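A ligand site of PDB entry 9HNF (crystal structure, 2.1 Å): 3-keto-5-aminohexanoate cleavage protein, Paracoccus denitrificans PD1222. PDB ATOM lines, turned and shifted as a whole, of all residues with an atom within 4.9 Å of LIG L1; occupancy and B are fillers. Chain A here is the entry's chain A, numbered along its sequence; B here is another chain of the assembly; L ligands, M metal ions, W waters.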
ATOM      1  N   ILE A  41      31.900 -20.233  32.227  1.00  0.00           N
ATOM      2  CA  ILE A  41      32.397 -21.108  31.178  1.00  0.00           C
ATOM      3  C   ILE A  41      32.300 -20.420  29.825  1.00  0.00           C
ATOM      4  O   ILE A  41      33.298 -20.249  29.124  1.00  0.00           O
ATOM      5  CB  ILE A  41      31.642 -22.449  31.174  1.00  0.00           C
ATOM      6  CG1 ILE A  41      31.838 -23.167  32.517  1.00  0.00           C
ATOM      7  CG2 ILE A  41      32.111 -23.316  30.023  1.00  0.00           C
ATOM      8  CD1 ILE A  41      33.289 -23.346  32.933  1.00  0.00           C
ATOM      9  N   HIS A  42      31.091 -20.023  29.434  1.00  0.00           N
ATOM     10  CA  HIS A  42      30.930 -19.233  28.228  1.00  0.00           C
ATOM     11  C   HIS A  42      31.691 -17.918  28.364  1.00  0.00           C
ATOM     12  O   HIS A  42      31.933 -17.424  29.465  1.00  0.00           O
ATOM     13  CB  HIS A  42      29.450 -18.958  27.944  1.00  0.00           C
ATOM     14  CG  HIS A  42      28.652 -20.182  27.616  1.00  0.00           C
ATOM     15  ND1 HIS A  42      27.377 -20.381  28.074  1.00  0.00           N
ATOM     16  CD2 HIS A  42      28.962 -21.265  26.857  1.00  0.00           C
ATOM     17  CE1 HIS A  42      26.921 -21.541  27.627  1.00  0.00           C
ATOM     18  NE2 HIS A  42      27.858 -22.096  26.887  1.00  0.00           N
ATOM     19  N   HIS A  75      27.073 -15.827  39.072  1.00  0.00           N
ATOM     20  CA  HIS A  75      28.485 -15.515  38.961  1.00  0.00           C
ATOM     21  C   HIS A  75      28.625 -14.025  38.663  1.00  0.00           C
ATOM     22  O   HIS A  75      27.659 -13.353  38.276  1.00  0.00           O
ATOM     23  CB  HIS A  75      29.184 -16.315  37.851  1.00  0.00           C
ATOM     24  CG  HIS A  75      29.263 -17.782  38.121  1.00  0.00           C
ATOM     25  ND1 HIS A  75      30.438 -18.491  37.999  1.00  0.00           N
ATOM     26  CD2 HIS A  75      28.307 -18.679  38.461  1.00  0.00           C
ATOM     27  CE1 HIS A  75      30.203 -19.766  38.268  1.00  0.00           C
ATOM     28  NE2 HIS A  75      28.924 -19.909  38.551  1.00  0.00           N
ATOM     29  N   GLY A 111      32.017 -22.275  42.882  1.00  0.00           N
ATOM     30  CA  GLY A 111      32.825 -22.886  41.849  1.00  0.00           C
ATOM     31  C   GLY A 111      33.642 -21.869  41.072  1.00  0.00           C
ATOM     32  O   GLY A 111      34.780 -22.145  40.699  1.00  0.00           O
ATOM     33  N   GLY A 112      33.062 -20.688  40.844  1.00  0.00           N
ATOM     34  CA  GLY A 112      33.734 -19.687  40.042  1.00  0.00           C
ATOM     35  C   GLY A 112      34.180 -20.262  38.722  1.00  0.00           C
ATOM     36  O   GLY A 112      33.513 -21.116  38.115  1.00  0.00           O
ATOM     37  N   PRO A 114      36.596 -22.793  36.832  1.00  0.00           N
ATOM     38  CA  PRO A 114      37.141 -24.072  37.341  1.00  0.00           C
ATOM     39  C   PRO A 114      38.653 -24.080  37.551  1.00  0.00           C
ATOM     40  O   PRO A 114      39.173 -25.064  38.074  1.00  0.00           O
ATOM     41  CB  PRO A 114      36.724 -25.091  36.270  1.00  0.00           C
ATOM     42  CG  PRO A 114      36.483 -24.283  35.035  1.00  0.00           C
ATOM     43  CD  PRO A 114      35.993 -22.939  35.502  1.00  0.00           C
ATOM     44  N   ASN A 136      30.579 -28.012  44.736  1.00  0.00           N
ATOM     45  CA  ASN A 136      30.992 -29.022  43.787  1.00  0.00           C
ATOM     46  C   ASN A 136      31.642 -30.185  44.524  1.00  0.00           C
ATOM     47  O   ASN A 136      32.476 -29.990  45.405  1.00  0.00           O
ATOM     48  CB  ASN A 136      31.932 -28.410  42.756  1.00  0.00           C
ATOM     49  CG  ASN A 136      31.295 -27.247  42.015  1.00  0.00           C
ATOM     50  OD1 ASN A 136      30.569 -27.435  41.046  1.00  0.00           O
ATOM     51  ND2 ASN A 136      31.548 -26.029  42.496  1.00  0.00           N
ATOM     52  N   PHE A 142      38.180 -30.467  33.470  1.00  0.00           N
ATOM     53  CA  PHE A 142      37.186 -29.547  32.869  1.00  0.00           C
ATOM     54  C   PHE A 142      37.724 -29.202  31.483  1.00  0.00           C
ATOM     55  O   PHE A 142      38.676 -28.426  31.374  1.00  0.00           O
ATOM     56  CB  PHE A 142      36.918 -28.329  33.759  1.00  0.00           C
ATOM     57  CG  PHE A 142      35.523 -27.770  33.658  1.00  0.00           C
ATOM     58  CD1 PHE A 142      35.028 -27.291  32.458  1.00  0.00           C
ATOM     59  CD2 PHE A 142      34.692 -27.738  34.768  1.00  0.00           C
ATOM     60  CE1 PHE A 142      33.740 -26.785  32.377  1.00  0.00           C
ATOM     61  CE2 PHE A 142      33.410 -27.237  34.682  1.00  0.00           C
ATOM     62  CZ  PHE A 142      32.930 -26.764  33.485  1.00  0.00           C
ATOM     63  N   MET A 147      34.702 -26.162  22.665  1.00  0.00           N
ATOM     64  CA  MET A 147      34.156 -24.823  22.318  1.00  0.00           C
ATOM     65  C   MET A 147      35.146 -24.087  21.421  1.00  0.00           C
ATOM     66  O   MET A 147      34.764 -23.084  20.811  1.00  0.00           O
ATOM     67  CB  MET A 147      33.898 -23.994  23.577  1.00  0.00           C
ATOM     68  CG  MET A 147      32.481 -24.113  24.108  1.00  0.00           C
ATOM     69  SD  MET A 147      32.277 -23.554  25.815  1.00  0.00           S
ATOM     70  CE  MET A 147      33.770 -24.220  26.555  1.00  0.00           C
ATOM     71  N   ARG A 150      34.171 -24.387  17.431  1.00  0.00           N
ATOM     72  CA  ARG A 150      33.144 -23.503  16.901  1.00  0.00           C
ATOM     73  C   ARG A 150      33.502 -22.030  17.034  1.00  0.00           C
ATOM     74  O   ARG A 150      33.068 -21.218  16.201  1.00  0.00           O
ATOM     75  CB  ARG A 150      31.806 -23.753  17.619  1.00  0.00           C
ATOM     76  CG  ARG A 150      30.659 -22.875  17.130  1.00  0.00           C
ATOM     77  CD  ARG A 150      29.471 -22.918  18.083  1.00  0.00           C
ATOM     78  NE  ARG A 150      28.771 -24.195  18.037  1.00  0.00           N
ATOM     79  CZ  ARG A 150      27.814 -24.488  17.165  1.00  0.00           C
ATOM     80  NH1 ARG A 150      27.445 -23.633  16.219  1.00  0.00           N
ATOM     81  NH2 ARG A 150      27.213 -25.670  17.243  1.00  0.00           N
ATOM     82  N   TYR A 151      34.277 -21.646  18.050  1.00  0.00           N
ATOM     83  CA  TYR A 151      34.415 -20.246  18.430  1.00  0.00           C
ATOM     84  C   TYR A 151      35.816 -19.674  18.277  1.00  0.00           C
ATOM     85  O   TYR A 151      35.991 -18.461  18.466  1.00  0.00           O
ATOM     86  CB  TYR A 151      33.976 -20.033  19.884  1.00  0.00           C
ATOM     87  CG  TYR A 151      32.488 -20.237  20.123  1.00  0.00           C
ATOM     88  CD1 TYR A 151      31.562 -19.421  19.502  1.00  0.00           C
ATOM     89  CD2 TYR A 151      32.031 -21.230  20.991  1.00  0.00           C
ATOM     90  CE1 TYR A 151      30.207 -19.591  19.719  1.00  0.00           C
ATOM     91  CE2 TYR A 151      30.679 -21.406  21.216  1.00  0.00           C
ATOM     92  CZ  TYR A 151      29.772 -20.578  20.585  1.00  0.00           C
ATOM     93  OH  TYR A 151      28.415 -20.742  20.795  1.00  0.00           O
ATOM     94  N   PHE A 171      39.428 -28.924  38.072  1.00  0.00           N
ATOM     95  CA  PHE A 171      38.423 -28.307  38.941  1.00  0.00           C
ATOM     96  C   PHE A 171      38.542 -28.990  40.293  1.00  0.00           C
ATOM     97  O   PHE A 171      38.045 -30.100  40.488  1.00  0.00           O
ATOM     98  CB  PHE A 171      37.034 -28.482  38.314  1.00  0.00           C
ATOM     99  CG  PHE A 171      35.935 -27.710  38.993  1.00  0.00           C
ATOM    100  CD1 PHE A 171      36.194 -26.573  39.745  1.00  0.00           C
ATOM    101  CD2 PHE A 171      34.616 -28.133  38.878  1.00  0.00           C
ATOM    102  CE1 PHE A 171      35.169 -25.876  40.347  1.00  0.00           C
ATOM    103  CE2 PHE A 171      33.593 -27.442  39.488  1.00  0.00           C
ATOM    104  CZ  PHE A 171      33.864 -26.316  40.228  1.00  0.00           C
ATOM    105  N   TYR A 197      28.604 -34.170  39.003  1.00  0.00           N
ATOM    106  CA  TYR A 197      28.886 -34.302  37.589  1.00  0.00           C
ATOM    107  C   TYR A 197      29.033 -35.760  37.152  1.00  0.00           C
ATOM    108  O   TYR A 197      29.212 -36.013  35.958  1.00  0.00           O
ATOM    109  CB  TYR A 197      30.169 -33.540  37.240  1.00  0.00           C
ATOM    110  CG  TYR A 197      30.118 -32.069  37.571  1.00  0.00           C
ATOM    111  CD1 TYR A 197      30.226 -31.630  38.884  1.00  0.00           C
ATOM    112  CD2 TYR A 197      29.976 -31.122  36.570  1.00  0.00           C
ATOM    113  CE1 TYR A 197      30.182 -30.279  39.185  1.00  0.00           C
ATOM    114  CE2 TYR A 197      29.922 -29.771  36.862  1.00  0.00           C
ATOM    115  CZ  TYR A 197      30.030 -29.350  38.174  1.00  0.00           C
ATOM    116  OH  TYR A 197      29.992 -28.004  38.469  1.00  0.00           O
ATOM    117  N   VAL A 223      24.619 -32.853  36.900  1.00  0.00           N
ATOM    118  CA  VAL A 223      25.035 -32.034  35.769  1.00  0.00           C
ATOM    119  C   VAL A 223      25.437 -32.946  34.614  1.00  0.00           C
ATOM    120  O   VAL A 223      26.287 -33.827  34.781  1.00  0.00           O
ATOM    121  CB  VAL A 223      26.209 -31.114  36.163  1.00  0.00           C
ATOM    122  CG1 VAL A 223      26.626 -30.241  34.982  1.00  0.00           C
ATOM    123  CG2 VAL A 223      25.846 -30.254  37.357  1.00  0.00           C
ATOM    124  N   LEU A 226      29.042 -32.192  30.290  1.00  0.00           N
ATOM    125  CA  LEU A 226      30.315 -31.495  30.318  1.00  0.00           C
ATOM    126  C   LEU A 226      31.455 -32.417  29.925  1.00  0.00           C
ATOM    127  O   LEU A 226      31.423 -33.624  30.193  1.00  0.00           O
ATOM    128  CB  LEU A 226      30.588 -30.909  31.700  1.00  0.00           C
ATOM    129  CG  LEU A 226      29.586 -29.887  32.249  1.00  0.00           C
ATOM    130  CD1 LEU A 226      30.224 -29.096  33.382  1.00  0.00           C
ATOM    131  CD2 LEU A 226      29.095 -28.959  31.147  1.00  0.00           C
ATOM    132  N   LEU A 257      20.815 -30.271  35.283  1.00  0.00           N
ATOM    133  CA  LEU A 257      21.406 -29.274  34.422  1.00  0.00           C
ATOM    134  C   LEU A 257      21.842 -29.977  33.148  1.00  0.00           C
ATOM    135  O   LEU A 257      22.703 -30.861  33.194  1.00  0.00           O
ATOM    136  CB  LEU A 257      22.589 -28.586  35.099  1.00  0.00           C
ATOM    137  CG  LEU A 257      23.295 -27.420  34.427  1.00  0.00           C
ATOM    138  CD1 LEU A 257      24.302 -26.835  35.406  1.00  0.00           C
ATOM    139  CD2 LEU A 257      23.989 -27.823  33.134  1.00  0.00           C
ATOM    140  N   ALA A 259      23.608 -29.428  29.504  1.00  0.00           N
ATOM    141  CA  ALA A 259      24.450 -28.465  28.820  1.00  0.00           C
ATOM    142  C   ALA A 259      24.008 -28.281  27.379  1.00  0.00           C
ATOM    143  O   ALA A 259      23.575 -29.228  26.716  1.00  0.00           O
ATOM    144  CB  ALA A 259      25.908 -28.925  28.852  1.00  0.00           C
ATOM    145  N   GLY A 260      24.112 -27.052  26.890  1.00  0.00           N
ATOM    146  CA  GLY A 260      23.854 -26.789  25.486  1.00  0.00           C
ATOM    147  C   GLY A 260      22.458 -27.182  25.079  1.00  0.00           C
ATOM    148  O   GLY A 260      21.468 -26.879  25.756  1.00  0.00           O
ATOM    149  N   ARG A 261      22.346 -27.861  23.944  1.00  0.00           N
ATOM    150  CA  ARG A 261      21.059 -28.199  23.370  1.00  0.00           C
ATOM    151  C   ARG A 261      20.367 -29.354  24.098  1.00  0.00           C
ATOM    152  O   ARG A 261      19.245 -29.703  23.730  1.00  0.00           O
ATOM    153  CB  ARG A 261      21.213 -28.531  21.889  1.00  0.00           C
ATOM    154  CG  ARG A 261      22.156 -29.691  21.585  1.00  0.00           C
ATOM    155  CD  ARG A 261      22.242 -29.924  20.094  1.00  0.00           C
ATOM    156  NE  ARG A 261      20.913 -30.036  19.499  1.00  0.00           N
ATOM    157  CZ  ARG A 261      20.663 -29.949  18.203  1.00  0.00           C
ATOM    158  NH1 ARG A 261      21.627 -29.762  17.317  1.00  0.00           N
ATOM    159  NH2 ARG A 261      19.407 -30.053  17.774  1.00  0.00           N
ATOM    160  N   ARG A 278      17.080 -26.574  35.984  1.00  0.00           N
ATOM    161  CA  ARG A 278      17.926 -25.399  35.862  1.00  0.00           C
ATOM    162  C   ARG A 278      18.066 -25.044  34.384  1.00  0.00           C
ATOM    163  O   ARG A 278      18.345 -25.917  33.562  1.00  0.00           O
ATOM    164  CB  ARG A 278      19.307 -25.634  36.486  1.00  0.00           C
ATOM    165  CG  ARG A 278      20.362 -24.626  36.051  1.00  0.00           C
ATOM    166  CD  ARG A 278      21.620 -24.710  36.902  1.00  0.00           C
ATOM    167  NE  ARG A 278      22.789 -24.239  36.179  1.00  0.00           N
ATOM    168  CZ  ARG A 278      23.954 -23.917  36.734  1.00  0.00           C
ATOM    169  NH1 ARG A 278      24.134 -23.982  38.041  1.00  0.00           N
ATOM    170  NH2 ARG A 278      24.954 -23.525  35.957  1.00  0.00           N
ATOM    171  N   GLU A 282      24.262 -19.449  31.436  1.00  0.00           N
ATOM    172  CA  GLU A 282      25.474 -20.091  31.947  1.00  0.00           C
ATOM    173  C   GLU A 282      25.694 -21.441  31.291  1.00  0.00           C
ATOM    174  O   GLU A 282      26.837 -21.889  31.158  1.00  0.00           O
ATOM    175  CB  GLU A 282      25.397 -20.251  33.469  1.00  0.00           C
ATOM    176  CG  GLU A 282      26.473 -21.166  34.077  1.00  0.00           C
ATOM    177  CD  GLU A 282      26.643 -20.980  35.592  1.00  0.00           C
ATOM    178  OE1 GLU A 282      26.028 -20.042  36.141  1.00  0.00           O
ATOM    179  OE2 GLU A 282      27.391 -21.749  36.232  1.00  0.00           O
ATOM    180  N   ASP A 283      24.614 -22.106  30.861  1.00  0.00           N
ATOM    181  CA  ASP A 283      24.673 -23.482  30.395  1.00  0.00           C
ATOM    182  C   ASP A 283      24.345 -23.656  28.919  1.00  0.00           C
ATOM    183  O   ASP A 283      24.743 -24.662  28.325  1.00  0.00           O
ATOM    184  CB  ASP A 283      23.694 -24.355  31.198  1.00  0.00           C
ATOM    185  CG  ASP A 283      23.901 -24.233  32.692  1.00  0.00           C
ATOM    186  OD1 ASP A 283      25.059 -24.058  33.110  1.00  0.00           O
ATOM    187  OD2 ASP A 283      22.908 -24.307  33.441  1.00  0.00           O
ATOM    188  N   ASN A 284      23.614 -22.715  28.316  1.00  0.00           N
ATOM    189  CA  ASN A 284      23.153 -22.884  26.943  1.00  0.00           C
ATOM    190  C   ASN A 284      22.936 -21.501  26.349  1.00  0.00           C
ATOM    191  O   ASN A 284      22.180 -20.706  26.915  1.00  0.00           O
ATOM    192  CB  ASN A 284      21.867 -23.713  26.895  1.00  0.00           C
ATOM    193  CG  ASN A 284      21.309 -23.858  25.489  1.00  0.00           C
ATOM    194  OD1 ASN A 284      22.059 -23.847  24.512  1.00  0.00           O
ATOM    195  ND2 ASN A 284      19.988 -23.986  25.394  1.00  0.00           N
ATOM    196  N   TRP A 286      21.689 -21.017  23.290  1.00  0.00           N
ATOM    197  CA  TRP A 286      20.782 -21.154  22.164  1.00  0.00           C
ATOM    198  C   TRP A 286      19.331 -21.161  22.622  1.00  0.00           C
ATOM    199  O   TRP A 286      19.008 -21.640  23.720  1.00  0.00           O
ATOM    200  CB  TRP A 286      21.104 -22.444  21.397  1.00  0.00           C
ATOM    201  CG  TRP A 286      22.473 -22.417  20.822  1.00  0.00           C
ATOM    202  CD1 TRP A 286      23.621 -22.830  21.423  1.00  0.00           C
ATOM    203  CD2 TRP A 286      22.857 -21.900  19.544  1.00  0.00           C
ATOM    204  NE1 TRP A 286      24.694 -22.621  20.588  1.00  0.00           N
ATOM    205  CE2 TRP A 286      24.255 -22.045  19.434  1.00  0.00           C
ATOM    206  CE3 TRP A 286      22.149 -21.336  18.478  1.00  0.00           C
ATOM    207  CZ2 TRP A 286      24.955 -21.654  18.298  1.00  0.00           C
ATOM    208  CZ3 TRP A 286      22.851 -20.934  17.350  1.00  0.00           C
ATOM    209  CH2 TRP A 286      24.241 -21.096  17.267  1.00  0.00           C
ATOM    210  N   ALA A 287      18.475 -20.601  21.773  1.00  0.00           N
ATOM    211  CA  ALA A 287      17.032 -20.694  21.931  1.00  0.00           C
ATOM    212  C   ALA A 287      16.379 -21.615  20.909  1.00  0.00           C
ATOM    213  O   ALA A 287      15.245 -22.040  21.129  1.00  0.00           O
ATOM    214  CB  ALA A 287      16.398 -19.301  21.803  1.00  0.00           C
ATOM    215  N   GLY A 288      17.062 -21.924  19.820  1.00  0.00           N
ATOM    216  CA  GLY A 288      16.511 -22.776  18.797  1.00  0.00           C
ATOM    217  C   GLY A 288      17.534 -23.036  17.720  1.00  0.00           C
ATOM    218  O   GLY A 288      18.728 -22.787  17.914  1.00  0.00           O
ATOM    219  N   LYS A 289      17.062 -23.528  16.579  1.00  0.00           N
ATOM    220  CA  LYS A 289      17.958 -23.792  15.467  1.00  0.00           C
ATOM    221  C   LYS A 289      18.417 -22.487  14.826  1.00  0.00           C
ATOM    222  O   LYS A 289      17.595 -21.659  14.431  1.00  0.00           O
ATOM    223  CB  LYS A 289      17.272 -24.678  14.429  1.00  0.00           C
ATOM    224  CG  LYS A 289      18.169 -25.079  13.264  1.00  0.00           C
ATOM    225  CD  LYS A 289      17.436 -25.924  12.243  1.00  0.00           C
ATOM    226  CE  LYS A 289      17.114 -27.320  12.765  1.00  0.00           C
ATOM    227  NZ  LYS A 289      18.334 -28.124  13.034  1.00  0.00           N
ATOM    228  N   GLY A 290      19.736 -22.313  14.724  1.00  0.00           N
ATOM    229  CA  GLY A 290      20.289 -21.108  14.136  1.00  0.00           C
ATOM    230  C   GLY A 290      19.883 -19.834  14.836  1.00  0.00           C
ATOM    231  O   GLY A 290      19.864 -18.769  14.215  1.00  0.00           O
ATOM    232  N   ARG A 291      19.561 -19.912  16.124  1.00  0.00           N
ATOM    233  CA  ARG A 291      19.009 -18.781  16.856  1.00  0.00           C
ATOM    234  C   ARG A 291      19.609 -18.746  18.256  1.00  0.00           C
ATOM    235  O   ARG A 291      19.383 -19.663  19.056  1.00  0.00           O
ATOM    236  CB  ARG A 291      17.488 -18.878  16.942  1.00  0.00           C
ATOM    237  CG  ARG A 291      16.769 -17.559  16.767  1.00  0.00           C
ATOM    238  CD  ARG A 291      15.460 -17.557  17.543  1.00  0.00           C
ATOM    239  NE  ARG A 291      14.761 -18.832  17.445  1.00  0.00           N
ATOM    240  CZ  ARG A 291      13.853 -19.250  18.320  1.00  0.00           C
ATOM    241  NH1 ARG A 291      13.498 -18.514  19.353  1.00  0.00           N
ATOM    242  NH2 ARG A 291      13.292 -20.439  18.137  1.00  0.00           N
ATOM    243  N   LEU B 310       9.781 -27.721  24.383  1.00  0.00           N
ATOM    244  CA  LEU B 310      11.082 -28.353  24.157  1.00  0.00           C
ATOM    245  C   LEU B 310      11.815 -27.789  22.952  1.00  0.00           C
ATOM    246  O   LEU B 310      12.966 -28.189  22.712  1.00  0.00           O
ATOM    247  CB  LEU B 310      10.898 -29.867  23.959  1.00  0.00           C
ATOM    248  CG  LEU B 310      10.754 -30.742  25.207  1.00  0.00           C
ATOM    249  CD1 LEU B 310      10.277 -32.123  24.815  1.00  0.00           C
ATOM    250  CD2 LEU B 310      12.081 -30.830  25.958  1.00  0.00           C
ATOM    251  N   GLY B 311      11.202 -26.896  22.190  1.00  0.00           N
ATOM    252  CA  GLY B 311      11.807 -26.411  20.971  1.00  0.00           C
ATOM    253  C   GLY B 311      11.620 -27.314  19.774  1.00  0.00           C
ATOM    254  O   GLY B 311      12.320 -27.157  18.779  1.00  0.00           O
HETATM  255  N1  LIG L   1      16.374 -26.965  18.118  1.00  0.00           N
HETATM  256  C1  LIG L   1      17.279 -27.273  17.177  1.00  0.00           C
HETATM  257  N2  LIG L   1      18.581 -27.014  17.145  1.00  0.00           N
HETATM  258  C2  LIG L   1      18.955 -26.353  18.248  1.00  0.00           C
HETATM  259  C3  LIG L   1      18.152 -25.967  19.299  1.00  0.00           C
HETATM  260  C4  LIG L   1      16.786 -26.304  19.224  1.00  0.00           C
HETATM  261  N3  LIG L   1      15.890 -26.001  20.146  1.00  0.00           N
HETATM  262  N4  LIG L   1      18.905 -25.300  20.255  1.00  0.00           N
HETATM  263  C5  LIG L   1      20.124 -25.297  19.778  1.00  0.00           C
HETATM  264  N5  LIG L   1      20.216 -25.929  18.560  1.00  0.00           N
HETATM  265  C6  LIG L   1      21.393 -26.114  17.731  1.00  0.00           C
HETATM  266  C7  LIG L   1      22.006 -24.829  17.175  1.00  0.00           C
HETATM  267  O1  LIG L   1      21.324 -24.361  16.041  1.00  0.00           O
HETATM  268  C8  LIG L   1      23.410 -25.327  16.869  1.00  0.00           C
HETATM  269  O2  LIG L   1      23.354 -26.121  15.695  1.00  0.00           O
HETATM  270  P1  LIG L   1      24.738 -26.187  14.902  1.00  0.00           P
HETATM  271  O3  LIG L   1      25.739 -26.956  15.721  1.00  0.00           O
HETATM  272  O4  LIG L   1      25.187 -24.798  14.612  1.00  0.00           O
HETATM  273  O5  LIG L   1      24.382 -26.920  13.649  1.00  0.00           O
HETATM  274  C9  LIG L   1      23.698 -26.176  18.087  1.00  0.00           C
HETATM  275  O6  LIG L   1      22.412 -26.697  18.506  1.00  0.00           O
HETATM  276  C10 LIG L   1      24.311 -25.425  19.234  1.00  0.00           C
HETATM  277  O7  LIG L   1      23.996 -26.108  20.469  1.00  0.00           O
HETATM  278  P2  LIG L   1      25.126 -27.042  21.113  1.00  0.00           P
HETATM  279  O8  LIG L   1      25.369 -28.201  20.210  1.00  0.00           O
HETATM  280  O9  LIG L   1      24.795 -27.319  22.535  1.00  0.00           O
HETATM  281  O10 LIG L   1      26.390 -26.066  21.049  1.00  0.00           O
HETATM  282  P3  LIG L   1      27.968 -26.322  20.986  1.00  0.00           P
HETATM  283  O11 LIG L   1      28.233 -27.501  20.140  1.00  0.00           O
HETATM  284  O12 LIG L   1      28.611 -25.025  20.651  1.00  0.00           O
HETATM  285  O13 LIG L   1      28.301 -26.721  22.511  1.00  0.00           O
HETATM  286  C11 LIG L   1      28.595 -26.324  24.876  1.00  0.00           C
HETATM  287  C12 LIG L   1      28.063 -25.767  23.564  1.00  0.00           C
HETATM  288  C13 LIG L   1      27.733 -27.519  25.322  1.00  0.00           C
HETATM  289  C14 LIG L   1      30.026 -26.814  24.673  1.00  0.00           C
HETATM  290  C15 LIG L   1      28.557 -25.233  25.943  1.00  0.00           C
HETATM  291  O14 LIG L   1      27.337 -24.553  25.810  1.00  0.00           O
HETATM  292  C16 LIG L   1      28.686 -25.761  27.358  1.00  0.00           C
HETATM  293  O15 LIG L   1      29.711 -26.330  27.718  1.00  0.00           O
HETATM  294  N6  LIG L   1      27.632 -25.593  28.154  1.00  0.00           N
HETATM  295  C17 LIG L   1      27.653 -25.793  29.606  1.00  0.00           C
HETATM  296  C18 LIG L   1      28.635 -24.884  30.300  1.00  0.00           C
HETATM  297  C19 LIG L   1      28.854 -25.332  31.727  1.00  0.00           C
HETATM  298  O16 LIG L   1      29.903 -25.889  32.064  1.00  0.00           O
HETATM  299  N7  LIG L   1      27.899 -25.057  32.617  1.00  0.00           N
HETATM  300  C20 LIG L   1      27.836 -25.680  33.921  1.00  0.00           C
HETATM  301  C21 LIG L   1      28.359 -24.760  35.004  1.00  0.00           C
HETATM  302  S1  LIG L   1      29.811 -25.360  35.896  1.00  0.00           S
HETATM  303  C22 LIG L   1      30.544 -24.103  36.858  1.00  0.00           C
HETATM  304  O17 LIG L   1      30.013 -23.047  37.037  1.00  0.00           O
HETATM  305  C23 LIG L   1      31.862 -24.482  37.441  1.00  0.00           C
HETATM  306  O1  LG2 L   2      28.772 -22.565  39.877  1.00  0.00           O
HETATM  307  C1  LG2 L   2      29.073 -23.680  40.345  1.00  0.00           C
HETATM  308  O2  LG2 L   2      29.672 -23.811  41.412  1.00  0.00           O
HETATM  309  C2  LG2 L   2      28.654 -24.961  39.628  1.00  0.00           C
HETATM  310  C3  LG2 L   2      27.625 -24.879  38.510  1.00  0.00           C
HETATM  311  O3  LG2 L   2      27.189 -23.827  38.055  1.00  0.00           O
HETATM  312  C4  LG2 L   2      27.143 -26.204  37.994  1.00  0.00           C
HETATM  313 ZN    ZN M   1      27.780 -21.853  38.239  1.00  0.00          ZN
HETATM  314  O   HOH W   1      30.027 -21.523  34.918  1.00  0.00           O
HETATM  315  O   HOH W   2      27.314 -23.125  21.797  1.00  0.00           O
HETATM  316  O   HOH W   3      25.548 -23.247  23.875  1.00  0.00           O
HETATM  317  O   HOH W   4      18.375 -25.161  22.745  1.00  0.00           O
HETATM  318  O   HOH W   5      31.294 -26.700  29.705  1.00  0.00           O
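OE2 of Glu 282 sits close to O17 of LIG L1, at 3.0 Å. A nitrogen (N4) of LIG L1 lies close to the backbone carbonyl oxygen (O) of Gly 288. Residues that only touch LIG L1: Trp 286, Gly 260, Leu 226, Ile 41, Phe 142, Lys 289, His 75, Ala 259, Met 147, Arg 278, Gly 112, Phe 171 and Gly 311 of chain B. Within 4 Å of LIG L1: Ile 41, His 42, His 75, Gly 112, Phe 142, Met 147, Arg 150, Phe 171, Tyr 197, Leu 226, Ala 259, Gly 260, Arg 261, Arg 278, Glu 282, Asp 283, Trp 286, Gly 288, Lys 289, Gly 290 and Gly 311 of chain B. The nearest printed residue that does not touch LIG L1 is Leu 257 (4.004 Å).
Water W4 lies within hydrogen-bond range of N4 of LIG L1 (2.5 Å) and ND2 of Asn 284 (3.3 Å). Water W2 lies within hydrogen-bond range of an oxygen (O12) of LIG L1 (2.6 Å), the side-chain hydroxyl (OH) of Tyr 151 (2.8 Å) and the indole nitrogen (NE1) of Trp 286 (2.9 Å). Water W3 lies within hydrogen-bond range of an oxygen (O14) of LIG L1 and the indole nitrogen of Trp 286.
The backbone NH of Arg 261 lies within hydrogen-bond range of an oxygen (O9) of LIG L1 (2.9 Å). ND2 of Asn 136 sits at hydrogen-bond distance from O2 of LG2 L2 (3.1 Å). O1 of LIG L1 lies within hydrogen-bond range of N of Gly 290, 2.9 Å away. NH2 of Arg 261 is in hydrogen-bond range of N2 of LIG L1, at 3.2 Å. The backbone NH (N) of Gly 111 is in hydrogen-bond range of an oxygen (O2) of LG2 L2. The backbone carbonyl oxygen (O) of Asp 283 sits at hydrogen-bond distance from a nitrogen (N6) of LIG L1 (3.0 Å). NE2 of His 42 is in hydrogen-bond range of O14 of LIG L1, 2.7 Å away. An oxygen (O3) of LIG L1 lies within salt-bridge range of the guanidinium group of Arg 150, at 2.5 Å. A sulfur (S1) of LIG L1 sits close to the side-chain hydroxyl of Tyr 197 (3.7 Å). N7 of LIG L1 is in hydrogen-bond range of OD1 of Asp 283, 3.1 Å away. O3 of LG2 L2 sits close to NH1 of Arg 278, 3.1 Å away.
The side-chain carboxylate (OE1) of Glu 282 lies within salt-bridge range of the guanidinium group (NH2) of Arg 278. The side-chain carboxylate of Asp 283 is in salt-bridge range of the guanidinium group of Arg 278 (2.7 Å). The backbone carbonyl oxygen (O) of Gly 260 sits close to the side-chain amide nitrogen (ND2) of Asn 284. OH of Tyr 197 is in hydrogen-bond range of OD1 of Asn 136 (2.7 Å). The backbone carbonyl oxygen (O) of Asp 283 sits at hydrogen-bond distance from the backbone NH (N) of Gly 260 (2.9 Å). A ring nitrogen (ND1) of His 42 lies within hydrogen-bond range of the backbone carbonyl oxygen (O) of Glu 282 (3.5 Å). The backbone carbonyl oxygen (O) of Trp 286 lies within hydrogen-bond range of the side-chain amide nitrogen (ND2) of Asn 284 (3.0 Å).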
